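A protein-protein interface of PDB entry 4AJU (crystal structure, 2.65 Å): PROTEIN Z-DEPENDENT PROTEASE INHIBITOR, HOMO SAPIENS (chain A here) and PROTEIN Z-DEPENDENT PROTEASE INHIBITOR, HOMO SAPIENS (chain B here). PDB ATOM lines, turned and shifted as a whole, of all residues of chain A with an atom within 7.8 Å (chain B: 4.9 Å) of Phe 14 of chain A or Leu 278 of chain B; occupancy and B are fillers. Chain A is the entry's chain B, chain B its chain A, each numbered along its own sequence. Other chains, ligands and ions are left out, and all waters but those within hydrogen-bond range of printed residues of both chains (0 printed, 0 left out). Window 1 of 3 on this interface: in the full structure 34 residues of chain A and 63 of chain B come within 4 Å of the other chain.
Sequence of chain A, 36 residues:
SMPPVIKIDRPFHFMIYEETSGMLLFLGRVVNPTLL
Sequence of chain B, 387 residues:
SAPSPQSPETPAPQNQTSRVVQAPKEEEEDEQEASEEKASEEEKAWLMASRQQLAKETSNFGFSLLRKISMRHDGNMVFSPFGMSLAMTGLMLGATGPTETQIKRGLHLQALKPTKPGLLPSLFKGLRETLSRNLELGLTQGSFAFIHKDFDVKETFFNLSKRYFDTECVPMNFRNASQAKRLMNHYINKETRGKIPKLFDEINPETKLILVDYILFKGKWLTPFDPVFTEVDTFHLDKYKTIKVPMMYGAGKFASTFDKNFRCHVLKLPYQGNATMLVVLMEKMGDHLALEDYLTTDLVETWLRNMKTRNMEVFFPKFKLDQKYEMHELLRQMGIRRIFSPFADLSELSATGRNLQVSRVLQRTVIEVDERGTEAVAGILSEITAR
Among the printed residues, pairs that only touch across the chains: Phe 12 of chain A with Val 279 of chain B, Phe 12 of chain A with Val 280 of chain B, Phe 12 of chain A with Phe 319 of chain B, His 13 of chain A with Leu 278 of chain B, His 13 of chain A with Val 279 of chain B, Phe 14 of chain A with Val 78 of chain B, Phe 14 of chain A with Leu 278 of chain B, Phe 14 of chain A with Ile 367 of chain B, Met 15 of chain A with Thr 276 of chain B, Met 15 of chain A with Met 277 of chain B, Ile 16 of chain A with Thr 276 of chain B, Tyr 17 of chain A with Leu 278 of chain B, Glu 19 of chain A with Thr 276 of chain B, Leu 27 of chain A with Val 78 of chain B, Gly 28 of chain A with Met 77 of chain B, Val 30 of chain A with Phe 319 of chain B and Val 30 of chain A with Leu 321 of chain B.
O of Leu 267 of chain B is in hydrogen-bond range of N of Val 279 of chain B, 2.9 Å away. The backbone carbonyl oxygen (O) of Ile 367 of chain B sits at hydrogen-bond distance from the backbone NH (N) of Leu 321 of chain B (2.9 Å). The backbone NH (N) of Val 30 of chain A lies within hydrogen-bond range of the backbone carbonyl oxygen (O) of Phe 12 of chain A, at 2.8 Å. O of Gly 28 of chain A lies within hydrogen-bond range of N of Phe 14 of chain A. N of Ile 16 of chain A is in hydrogen-bond range of O of Phe 26 of chain A, at 2.8 Å.
Phe 14 of chain A touches just these residues of chain B: Val 78 (3.7 Å), Leu 278 (3.2 Å) and Ile 367 (3.6 Å). Of the printed residues of chain B, Ile 16 of chain A touches Thr 276. Leu 24 of chain A touches none of the printed residues of chain B. Of the printed residues of chain A, Val 78 of chain B touches Phe 14 and Leu 27. Leu 278 of chain B touches four residues of chain A. Of the printed residues of chain A, Val 279 of chain B touches Phe 12 and His 13. Printed residues of chain A within 4 Å of Val 280 of chain B: Phe 12 and His 13. The nearest residue of chain B that does not touch Phe 14 of chain A is Met 277 of chain B (4.05 Å). The nearest residue of chain A that does not touch Leu 278 of chain B is Ile 16 of chain A (5.0 Å).
The backbone carbonyl oxygen (O) of Arg 29 of chain A sits at hydrogen-bond distance from the backbone NH (N) of Met 77 of chain B. NZ of Lys 268 of chain B lies within salt-bridge range of OE1 of Glu 19 of chain A, 3.7 Å away. The backbone NH of Tyr 17 of chain A sits at hydrogen-bond distance from the backbone carbonyl oxygen of Thr 276 of chain B (2.9 Å). The backbone carbonyl oxygen of Met 15 of chain A is in hydrogen-bond range of the backbone NH of Leu 278 of chain B. N of Val 280 of chain B sits at hydrogen-bond distance from O of His 13 of chain A, at 2.8 Å.
Of the 14 printed residues of chain A, 11 touch a printed residue of chain B. Hydrophobic or aromatic side chains of chain A within 4 Å of the printed part of chain B: Phe 12, Phe 14, Met 15, Ile 16, Tyr 17 and Val 30. Along chain A the printed residues that touch a printed residue of chain B span positions 12 to 30. Among the printed residues, 22 pairs touch across the chains.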
ATOM      1  N   PHE A  12      -1.050   7.184   4.396  1.00  0.00           N
ATOM      2  CA  PHE A  12      -0.297   7.188   3.146  1.00  0.00           C
ATOM      3  C   PHE A  12       1.197   7.142   3.367  1.00  0.00           C
ATOM      4  O   PHE A  12       1.680   7.435   4.451  1.00  0.00           O
ATOM      5  CB  PHE A  12      -0.647   8.431   2.322  1.00  0.00           C
ATOM      6  CG  PHE A  12      -0.292   9.730   2.992  1.00  0.00           C
ATOM      7  CD1 PHE A  12      -1.156  10.310   3.907  1.00  0.00           C
ATOM      8  CD2 PHE A  12       0.897  10.380   2.688  1.00  0.00           C
ATOM      9  CE1 PHE A  12      -0.840  11.503   4.524  1.00  0.00           C
ATOM     10  CE2 PHE A  12       1.230  11.583   3.294  1.00  0.00           C
ATOM     11  CZ  PHE A  12       0.360  12.146   4.223  1.00  0.00           C
ATOM     12  N   HIS A  13       1.918   6.783   2.315  1.00  0.00           N
ATOM     13  CA  HIS A  13       3.377   6.762   2.342  1.00  0.00           C
ATOM     14  C   HIS A  13       3.933   7.896   1.499  1.00  0.00           C
ATOM     15  O   HIS A  13       3.342   8.293   0.495  1.00  0.00           O
ATOM     16  CB  HIS A  13       3.890   5.426   1.807  1.00  0.00           C
ATOM     17  CG  HIS A  13       3.564   4.265   2.687  1.00  0.00           C
ATOM     18  ND1 HIS A  13       2.326   3.658   2.689  1.00  0.00           N
ATOM     19  CD2 HIS A  13       4.311   3.607   3.607  1.00  0.00           C
ATOM     20  CE1 HIS A  13       2.328   2.667   3.567  1.00  0.00           C
ATOM     21  NE2 HIS A  13       3.521   2.614   4.136  1.00  0.00           N
ATOM     22  N   PHE A  14       5.071   8.429   1.912  1.00  0.00           N
ATOM     23  CA  PHE A  14       5.675   9.517   1.171  1.00  0.00           C
ATOM     24  C   PHE A  14       7.155   9.278   0.983  1.00  0.00           C
ATOM     25  O   PHE A  14       7.783   8.585   1.776  1.00  0.00           O
ATOM     26  CB  PHE A  14       5.392  10.867   1.839  1.00  0.00           C
ATOM     27  CG  PHE A  14       6.107  11.079   3.138  1.00  0.00           C
ATOM     28  CD1 PHE A  14       7.403  11.580   3.161  1.00  0.00           C
ATOM     29  CD2 PHE A  14       5.475  10.815   4.344  1.00  0.00           C
ATOM     30  CE1 PHE A  14       8.067  11.792   4.370  1.00  0.00           C
ATOM     31  CE2 PHE A  14       6.139  11.022   5.562  1.00  0.00           C
ATOM     32  CZ  PHE A  14       7.431  11.516   5.568  1.00  0.00           C
ATOM     33  N   MET A  15       7.698   9.839  -0.090  1.00  0.00           N
ATOM     34  CA  MET A  15       9.105   9.667  -0.420  1.00  0.00           C
ATOM     35  C   MET A  15       9.624  10.965  -0.994  1.00  0.00           C
ATOM     36  O   MET A  15       9.036  11.483  -1.931  1.00  0.00           O
ATOM     37  CB  MET A  15       9.247   8.559  -1.462  1.00  0.00           C
ATOM     38  CG  MET A  15       8.467   7.304  -1.122  1.00  0.00           C
ATOM     39  SD  MET A  15       8.388   6.112  -2.464  1.00  0.00           S
ATOM     40  CE  MET A  15      10.133   5.803  -2.647  1.00  0.00           C
ATOM     41  N   ILE A  16      10.693  11.511  -0.435  1.00  0.00           N
ATOM     42  CA  ILE A  16      11.309  12.706  -1.021  1.00  0.00           C
ATOM     43  C   ILE A  16      12.578  12.320  -1.765  1.00  0.00           C
ATOM     44  O   ILE A  16      13.535  11.836  -1.162  1.00  0.00           O
ATOM     45  CB  ILE A  16      11.653  13.754   0.017  1.00  0.00           C
ATOM     46  CG1 ILE A  16      10.378  14.254   0.713  1.00  0.00           C
ATOM     47  CG2 ILE A  16      12.379  14.910  -0.645  1.00  0.00           C
ATOM     48  CD1 ILE A  16      10.641  15.193   1.877  1.00  0.00           C
ATOM     49  N   TYR A  17      12.568  12.539  -3.077  1.00  0.00           N
ATOM     50  CA  TYR A  17      13.649  12.137  -3.965  1.00  0.00           C
ATOM     51  C   TYR A  17      14.334  13.356  -4.544  1.00  0.00           C
ATOM     52  O   TYR A  17      13.661  14.340  -4.855  1.00  0.00           O
ATOM     53  CB  TYR A  17      13.088  11.366  -5.148  1.00  0.00           C
ATOM     54  CG  TYR A  17      13.022   9.878  -4.983  1.00  0.00           C
ATOM     55  CD1 TYR A  17      14.167   9.098  -5.108  1.00  0.00           C
ATOM     56  CD2 TYR A  17      11.810   9.239  -4.754  1.00  0.00           C
ATOM     57  CE1 TYR A  17      14.113   7.723  -4.981  1.00  0.00           C
ATOM     58  CE2 TYR A  17      11.741   7.867  -4.622  1.00  0.00           C
ATOM     59  CZ  TYR A  17      12.894   7.109  -4.735  1.00  0.00           C
ATOM     60  OH  TYR A  17      12.833   5.733  -4.619  1.00  0.00           O
ATOM     61  N   GLU A  19      15.844  14.273  -7.885  1.00  0.00           N
ATOM     62  CA  GLU A  19      15.543  13.609  -9.156  1.00  0.00           C
ATOM     63  C   GLU A  19      16.736  13.454 -10.088  1.00  0.00           C
ATOM     64  O   GLU A  19      16.739  12.564 -10.931  1.00  0.00           O
ATOM     65  CB  GLU A  19      14.398  14.324  -9.872  1.00  0.00           C
ATOM     66  CG  GLU A  19      13.110  14.414  -9.026  1.00  0.00           C
ATOM     67  CD  GLU A  19      11.945  15.015  -9.791  1.00  0.00           C
ATOM     68  OE1 GLU A  19      11.389  14.309 -10.658  1.00  0.00           O
ATOM     69  OE2 GLU A  19      11.584  16.187  -9.523  1.00  0.00           O
ATOM     70  N   LEU A  24      17.020   8.757  -2.550  1.00  0.00           N
ATOM     71  CA  LEU A  24      15.895   8.797  -1.632  1.00  0.00           C
ATOM     72  C   LEU A  24      16.342   9.518  -0.365  1.00  0.00           C
ATOM     73  O   LEU A  24      17.023   8.938   0.463  1.00  0.00           O
ATOM     74  CB  LEU A  24      15.436   7.370  -1.306  1.00  0.00           C
ATOM     75  CG  LEU A  24      14.162   7.219  -0.474  1.00  0.00           C
ATOM     76  CD1 LEU A  24      12.992   7.950  -1.136  1.00  0.00           C
ATOM     77  CD2 LEU A  24      13.843   5.747  -0.265  1.00  0.00           C
ATOM     78  N   PHE A  26      14.282  11.163   2.009  1.00  0.00           N
ATOM     79  CA  PHE A  26      13.401  10.860   3.131  1.00  0.00           C
ATOM     80  C   PHE A  26      12.314   9.893   2.713  1.00  0.00           C
ATOM     81  O   PHE A  26      11.856   9.911   1.569  1.00  0.00           O
ATOM     82  CB  PHE A  26      12.784  12.142   3.679  1.00  0.00           C
ATOM     83  CG  PHE A  26      13.779  13.032   4.334  1.00  0.00           C
ATOM     84  CD1 PHE A  26      14.086  12.877   5.674  1.00  0.00           C
ATOM     85  CD2 PHE A  26      14.455  13.992   3.603  1.00  0.00           C
ATOM     86  CE1 PHE A  26      15.018  13.678   6.279  1.00  0.00           C
ATOM     87  CE2 PHE A  26      15.399  14.802   4.207  1.00  0.00           C
ATOM     88  CZ  PHE A  26      15.676  14.647   5.542  1.00  0.00           C
ATOM     89  N   LEU A  27      11.909   9.055   3.659  1.00  0.00           N
ATOM     90  CA  LEU A  27      10.950   7.992   3.413  1.00  0.00           C
ATOM     91  C   LEU A  27      10.041   7.940   4.624  1.00  0.00           C
ATOM     92  O   LEU A  27      10.520   7.988   5.758  1.00  0.00           O
ATOM     93  CB  LEU A  27      11.695   6.660   3.239  1.00  0.00           C
ATOM     94  CG  LEU A  27      10.874   5.382   3.065  1.00  0.00           C
ATOM     95  CD1 LEU A  27       9.949   5.486   1.883  1.00  0.00           C
ATOM     96  CD2 LEU A  27      11.790   4.184   2.907  1.00  0.00           C
ATOM     97  N   GLY A  28       8.736   7.844   4.409  1.00  0.00           N
ATOM     98  CA  GLY A  28       7.828   7.832   5.551  1.00  0.00           C
ATOM     99  C   GLY A  28       6.416   7.342   5.336  1.00  0.00           C
ATOM    100  O   GLY A  28       5.983   7.105   4.211  1.00  0.00           O
ATOM    101  N   ARG A  29       5.721   7.190   6.461  1.00  0.00           N
ATOM    102  CA  ARG A  29       4.315   6.814   6.518  1.00  0.00           C
ATOM    103  C   ARG A  29       3.608   7.783   7.469  1.00  0.00           C
ATOM    104  O   ARG A  29       4.089   8.058   8.563  1.00  0.00           O
ATOM    105  CB  ARG A  29       4.190   5.388   7.038  1.00  0.00           C
ATOM    106  CG  ARG A  29       2.761   4.874   7.218  1.00  0.00           C
ATOM    107  CD  ARG A  29       2.744   3.415   7.717  1.00  0.00           C
ATOM    108  NE  ARG A  29       3.463   3.274   8.986  1.00  0.00           N
ATOM    109  CZ  ARG A  29       3.745   2.117   9.588  1.00  0.00           C
ATOM    110  NH1 ARG A  29       3.381   0.958   9.045  1.00  0.00           N
ATOM    111  NH2 ARG A  29       4.402   2.117  10.748  1.00  0.00           N
ATOM    112  N   VAL A  30       2.477   8.314   7.033  1.00  0.00           N
ATOM    113  CA  VAL A  30       1.635   9.156   7.868  1.00  0.00           C
ATOM    114  C   VAL A  30       0.322   8.417   8.087  1.00  0.00           C
ATOM    115  O   VAL A  30      -0.412   8.136   7.145  1.00  0.00           O
ATOM    116  CB  VAL A  30       1.388  10.518   7.206  1.00  0.00           C
ATOM    117  CG1 VAL A  30       0.321  11.297   7.959  1.00  0.00           C
ATOM    118  CG2 VAL A  30       2.701  11.316   7.130  1.00  0.00           C
ATOM    119  N   VAL A  31       0.064   8.075   9.339  1.00  0.00           N
ATOM    120  CA  VAL A  31      -1.122   7.316   9.739  1.00  0.00           C
ATOM    121  C   VAL A  31      -2.124   8.202  10.492  1.00  0.00           C
ATOM    122  O   VAL A  31      -3.298   7.855  10.609  1.00  0.00           O
ATOM    123  CB  VAL A  31      -0.698   6.114  10.625  1.00  0.00           C
ATOM    124  CG1 VAL A  31      -1.699   5.858  11.718  1.00  0.00           C
ATOM    125  CG2 VAL A  31      -0.474   4.874   9.773  1.00  0.00           C
ATOM    126  N   MET B  77       5.756   7.303  10.791  1.00  0.00           N
ATOM    127  CA  MET B  77       7.214   7.129  10.747  1.00  0.00           C
ATOM    128  C   MET B  77       7.902   7.962   9.680  1.00  0.00           C
ATOM    129  O   MET B  77       7.346   8.229   8.621  1.00  0.00           O
ATOM    130  CB  MET B  77       7.609   5.657  10.588  1.00  0.00           C
ATOM    131  CG  MET B  77       6.744   4.840   9.673  1.00  0.00           C
ATOM    132  SD  MET B  77       7.110   3.075   9.842  1.00  0.00           S
ATOM    133  CE  MET B  77       8.795   3.067   9.228  1.00  0.00           C
ATOM    134  N   VAL B  78       9.133   8.353   9.970  1.00  0.00           N
ATOM    135  CA  VAL B  78       9.949   9.073   9.013  1.00  0.00           C
ATOM    136  C   VAL B  78      11.434   8.796   9.268  1.00  0.00           C
ATOM    137  O   VAL B  78      11.863   8.693  10.406  1.00  0.00           O
ATOM    138  CB  VAL B  78       9.653  10.590   9.090  1.00  0.00           C
ATOM    139  CG1 VAL B  78      10.107  11.166  10.432  1.00  0.00           C
ATOM    140  CG2 VAL B  78      10.289  11.335   7.914  1.00  0.00           C
ATOM    141  N   VAL B 266      -0.727   7.089  -7.002  1.00  0.00           N
ATOM    142  CA  VAL B 266       0.596   7.663  -6.745  1.00  0.00           C
ATOM    143  C   VAL B 266       0.639   9.069  -7.332  1.00  0.00           C
ATOM    144  O   VAL B 266       0.279   9.252  -8.483  1.00  0.00           O
ATOM    145  CB  VAL B 266       1.704   6.814  -7.386  1.00  0.00           C
ATOM    146  CG1 VAL B 266       3.068   7.223  -6.833  1.00  0.00           C
ATOM    147  CG2 VAL B 266       1.430   5.325  -7.160  1.00  0.00           C
ATOM    148  N   LEU B 267       1.074  10.052  -6.550  1.00  0.00           N
ATOM    149  CA  LEU B 267       1.026  11.456  -6.971  1.00  0.00           C
ATOM    150  C   LEU B 267       2.375  12.166  -6.763  1.00  0.00           C
ATOM    151  O   LEU B 267       3.003  12.002  -5.721  1.00  0.00           O
ATOM    152  CB  LEU B 267      -0.088  12.169  -6.202  1.00  0.00           C
ATOM    153  CG  LEU B 267      -0.185  13.698  -6.236  1.00  0.00           C
ATOM    154  CD1 LEU B 267      -0.878  14.185  -7.477  1.00  0.00           C
ATOM    155  CD2 LEU B 267      -0.922  14.187  -5.017  1.00  0.00           C
ATOM    156  N   LYS B 268       2.814  12.941  -7.760  1.00  0.00           N
ATOM    157  CA  LYS B 268       4.051  13.734  -7.657  1.00  0.00           C
ATOM    158  C   LYS B 268       3.741  15.145  -7.187  1.00  0.00           C
ATOM    159  O   LYS B 268       2.912  15.843  -7.783  1.00  0.00           O
ATOM    160  CB  LYS B 268       4.792  13.817  -8.996  1.00  0.00           C
ATOM    161  CG  LYS B 268       5.388  12.495  -9.466  1.00  0.00           C
ATOM    162  CD  LYS B 268       6.088  12.603 -10.826  1.00  0.00           C
ATOM    163  CE  LYS B 268       7.431  13.338 -10.718  1.00  0.00           C
ATOM    164  NZ  LYS B 268       8.098  13.524 -12.053  1.00  0.00           N
ATOM    165  N   THR B 276      11.339  16.136  -5.523  1.00  0.00           N
ATOM    166  CA  THR B 276       9.914  15.845  -5.577  1.00  0.00           C
ATOM    167  C   THR B 276       9.460  14.935  -4.438  1.00  0.00           C
ATOM    168  O   THR B 276      10.249  14.156  -3.918  1.00  0.00           O
ATOM    169  CB  THR B 276       9.546  15.164  -6.892  1.00  0.00           C
ATOM    170  OG1 THR B 276       8.131  14.977  -6.939  1.00  0.00           O
ATOM    171  CG2 THR B 276      10.223  13.814  -6.998  1.00  0.00           C
ATOM    172  N   MET B 277       8.183  15.039  -4.069  1.00  0.00           N
ATOM    173  CA  MET B 277       7.582  14.130  -3.089  1.00  0.00           C
ATOM    174  C   MET B 277       6.645  13.185  -3.809  1.00  0.00           C
ATOM    175  O   MET B 277       5.710  13.641  -4.439  1.00  0.00           O
ATOM    176  CB  MET B 277       6.798  14.901  -2.018  1.00  0.00           C
ATOM    177  CG  MET B 277       6.190  13.985  -0.971  1.00  0.00           C
ATOM    178  SD  MET B 277       5.231  14.797   0.321  1.00  0.00           S
ATOM    179  CE  MET B 277       6.493  15.173   1.539  1.00  0.00           C
ATOM    180  N   LEU B 278       6.899  11.882  -3.737  1.00  0.00           N
ATOM    181  CA  LEU B 278       5.916  10.889  -4.185  1.00  0.00           C
ATOM    182  C   LEU B 278       4.997  10.608  -3.022  1.00  0.00           C
ATOM    183  O   LEU B 278       5.466  10.346  -1.909  1.00  0.00           O
ATOM    184  CB  LEU B 278       6.562   9.568  -4.563  1.00  0.00           C
ATOM    185  CG  LEU B 278       7.337   9.443  -5.859  1.00  0.00           C
ATOM    186  CD1 LEU B 278       7.990   8.055  -5.884  1.00  0.00           C
ATOM    187  CD2 LEU B 278       6.433   9.644  -7.077  1.00  0.00           C
ATOM    188  N   VAL B 279       3.699  10.638  -3.279  1.00  0.00           N
ATOM    189  CA  VAL B 279       2.714  10.261  -2.283  1.00  0.00           C
ATOM    190  C   VAL B 279       1.977   9.021  -2.775  1.00  0.00           C
ATOM    191  O   VAL B 279       1.496   8.993  -3.897  1.00  0.00           O
ATOM    192  CB  VAL B 279       1.739  11.416  -2.030  1.00  0.00           C
ATOM    193  CG1 VAL B 279       0.586  10.977  -1.141  1.00  0.00           C
ATOM    194  CG2 VAL B 279       2.494  12.586  -1.421  1.00  0.00           C
ATOM    195  N   VAL B 280       1.918   7.991  -1.940  1.00  0.00           N
ATOM    196  CA  VAL B 280       1.224   6.749  -2.284  1.00  0.00           C
ATOM    197  C   VAL B 280       0.031   6.537  -1.357  1.00  0.00           C
ATOM    198  O   VAL B 280       0.186   6.338  -0.152  1.00  0.00           O
ATOM    199  CB  VAL B 280       2.163   5.537  -2.207  1.00  0.00           C
ATOM    200  CG1 VAL B 280       1.447   4.276  -2.681  1.00  0.00           C
ATOM    201  CG2 VAL B 280       3.399   5.790  -3.035  1.00  0.00           C
ATOM    202  N   VAL B 300       8.635   1.488  -8.023  1.00  0.00           N
ATOM    203  CA  VAL B 300       8.648   2.945  -8.138  1.00  0.00           C
ATOM    204  C   VAL B 300       8.960   3.377  -9.571  1.00  0.00           C
ATOM    205  O   VAL B 300       8.352   4.317 -10.086  1.00  0.00           O
ATOM    206  CB  VAL B 300       9.653   3.578  -7.163  1.00  0.00           C
ATOM    207  CG1 VAL B 300       9.793   5.054  -7.429  1.00  0.00           C
ATOM    208  CG2 VAL B 300       9.207   3.342  -5.738  1.00  0.00           C
ATOM    209  N   LEU B 304       6.676   5.718 -12.053  1.00  0.00           N
ATOM    210  CA  LEU B 304       7.217   6.900 -12.731  1.00  0.00           C
ATOM    211  C   LEU B 304       7.073   6.811 -14.248  1.00  0.00           C
ATOM    212  O   LEU B 304       6.920   7.825 -14.925  1.00  0.00           O
ATOM    213  CB  LEU B 304       8.675   7.134 -12.347  1.00  0.00           C
ATOM    214  CG  LEU B 304       8.884   7.525 -10.880  1.00  0.00           C
ATOM    215  CD1 LEU B 304      10.364   7.650 -10.574  1.00  0.00           C
ATOM    216  CD2 LEU B 304       8.145   8.808 -10.500  1.00  0.00           C
ATOM    217  N   MET B 307       3.186   7.536 -15.185  1.00  0.00           N
ATOM    218  CA  MET B 307       2.622   8.838 -14.824  1.00  0.00           C
ATOM    219  C   MET B 307       2.007   9.504 -16.048  1.00  0.00           C
ATOM    220  O   MET B 307       2.479   9.317 -17.168  1.00  0.00           O
ATOM    221  CB  MET B 307       3.696   9.774 -14.261  1.00  0.00           C
ATOM    222  CG  MET B 307       4.231   9.394 -12.906  1.00  0.00           C
ATOM    223  SD  MET B 307       3.032   9.632 -11.589  1.00  0.00           S
ATOM    224  CE  MET B 307       3.964   9.149 -10.148  1.00  0.00           C
ATOM    225  N   PHE B 319       1.301  18.271   8.013  1.00  0.00           N
ATOM    226  CA  PHE B 319       1.730  17.421   9.126  1.00  0.00           C
ATOM    227  C   PHE B 319       3.136  17.756   9.619  1.00  0.00           C
ATOM    228  O   PHE B 319       3.979  18.207   8.838  1.00  0.00           O
ATOM    229  CB  PHE B 319       1.625  15.931   8.750  1.00  0.00           C
ATOM    230  CG  PHE B 319       2.425  15.540   7.536  1.00  0.00           C
ATOM    231  CD1 PHE B 319       1.875  15.626   6.271  1.00  0.00           C
ATOM    232  CD2 PHE B 319       3.729  15.066   7.664  1.00  0.00           C
ATOM    233  CE1 PHE B 319       2.612  15.262   5.149  1.00  0.00           C
ATOM    234  CE2 PHE B 319       4.477  14.697   6.550  1.00  0.00           C
ATOM    235  CZ  PHE B 319       3.915  14.788   5.294  1.00  0.00           C
ATOM    236  N   LEU B 321       6.079  15.552  11.815  1.00  0.00           N
ATOM    237  CA  LEU B 321       6.481  14.316  12.477  1.00  0.00           C
ATOM    238  C   LEU B 321       7.803  14.492  13.223  1.00  0.00           C
ATOM    239  O   LEU B 321       8.609  15.350  12.897  1.00  0.00           O
ATOM    240  CB  LEU B 321       6.604  13.170  11.474  1.00  0.00           C
ATOM    241  CG  LEU B 321       5.414  12.910  10.556  1.00  0.00           C
ATOM    242  CD1 LEU B 321       5.754  11.770   9.608  1.00  0.00           C
ATOM    243  CD2 LEU B 321       4.147  12.610  11.346  1.00  0.00           C
ATOM    244  N   ILE B 367      10.073  16.269  10.321  1.00  0.00           N
ATOM    245  CA  ILE B 367       9.583  16.781   9.054  1.00  0.00           C
ATOM    246  C   ILE B 367       8.365  17.674   9.293  1.00  0.00           C
ATOM    247  O   ILE B 367       7.581  17.436  10.205  1.00  0.00           O
ATOM    248  CB  ILE B 367       9.253  15.622   8.097  1.00  0.00           C
ATOM    249  CG1 ILE B 367       8.914  16.149   6.702  1.00  0.00           C
ATOM    250  CG2 ILE B 367       8.137  14.763   8.664  1.00  0.00           C
ATOM    251  CD1 ILE B 367       8.501  15.063   5.731  1.00  0.00           C
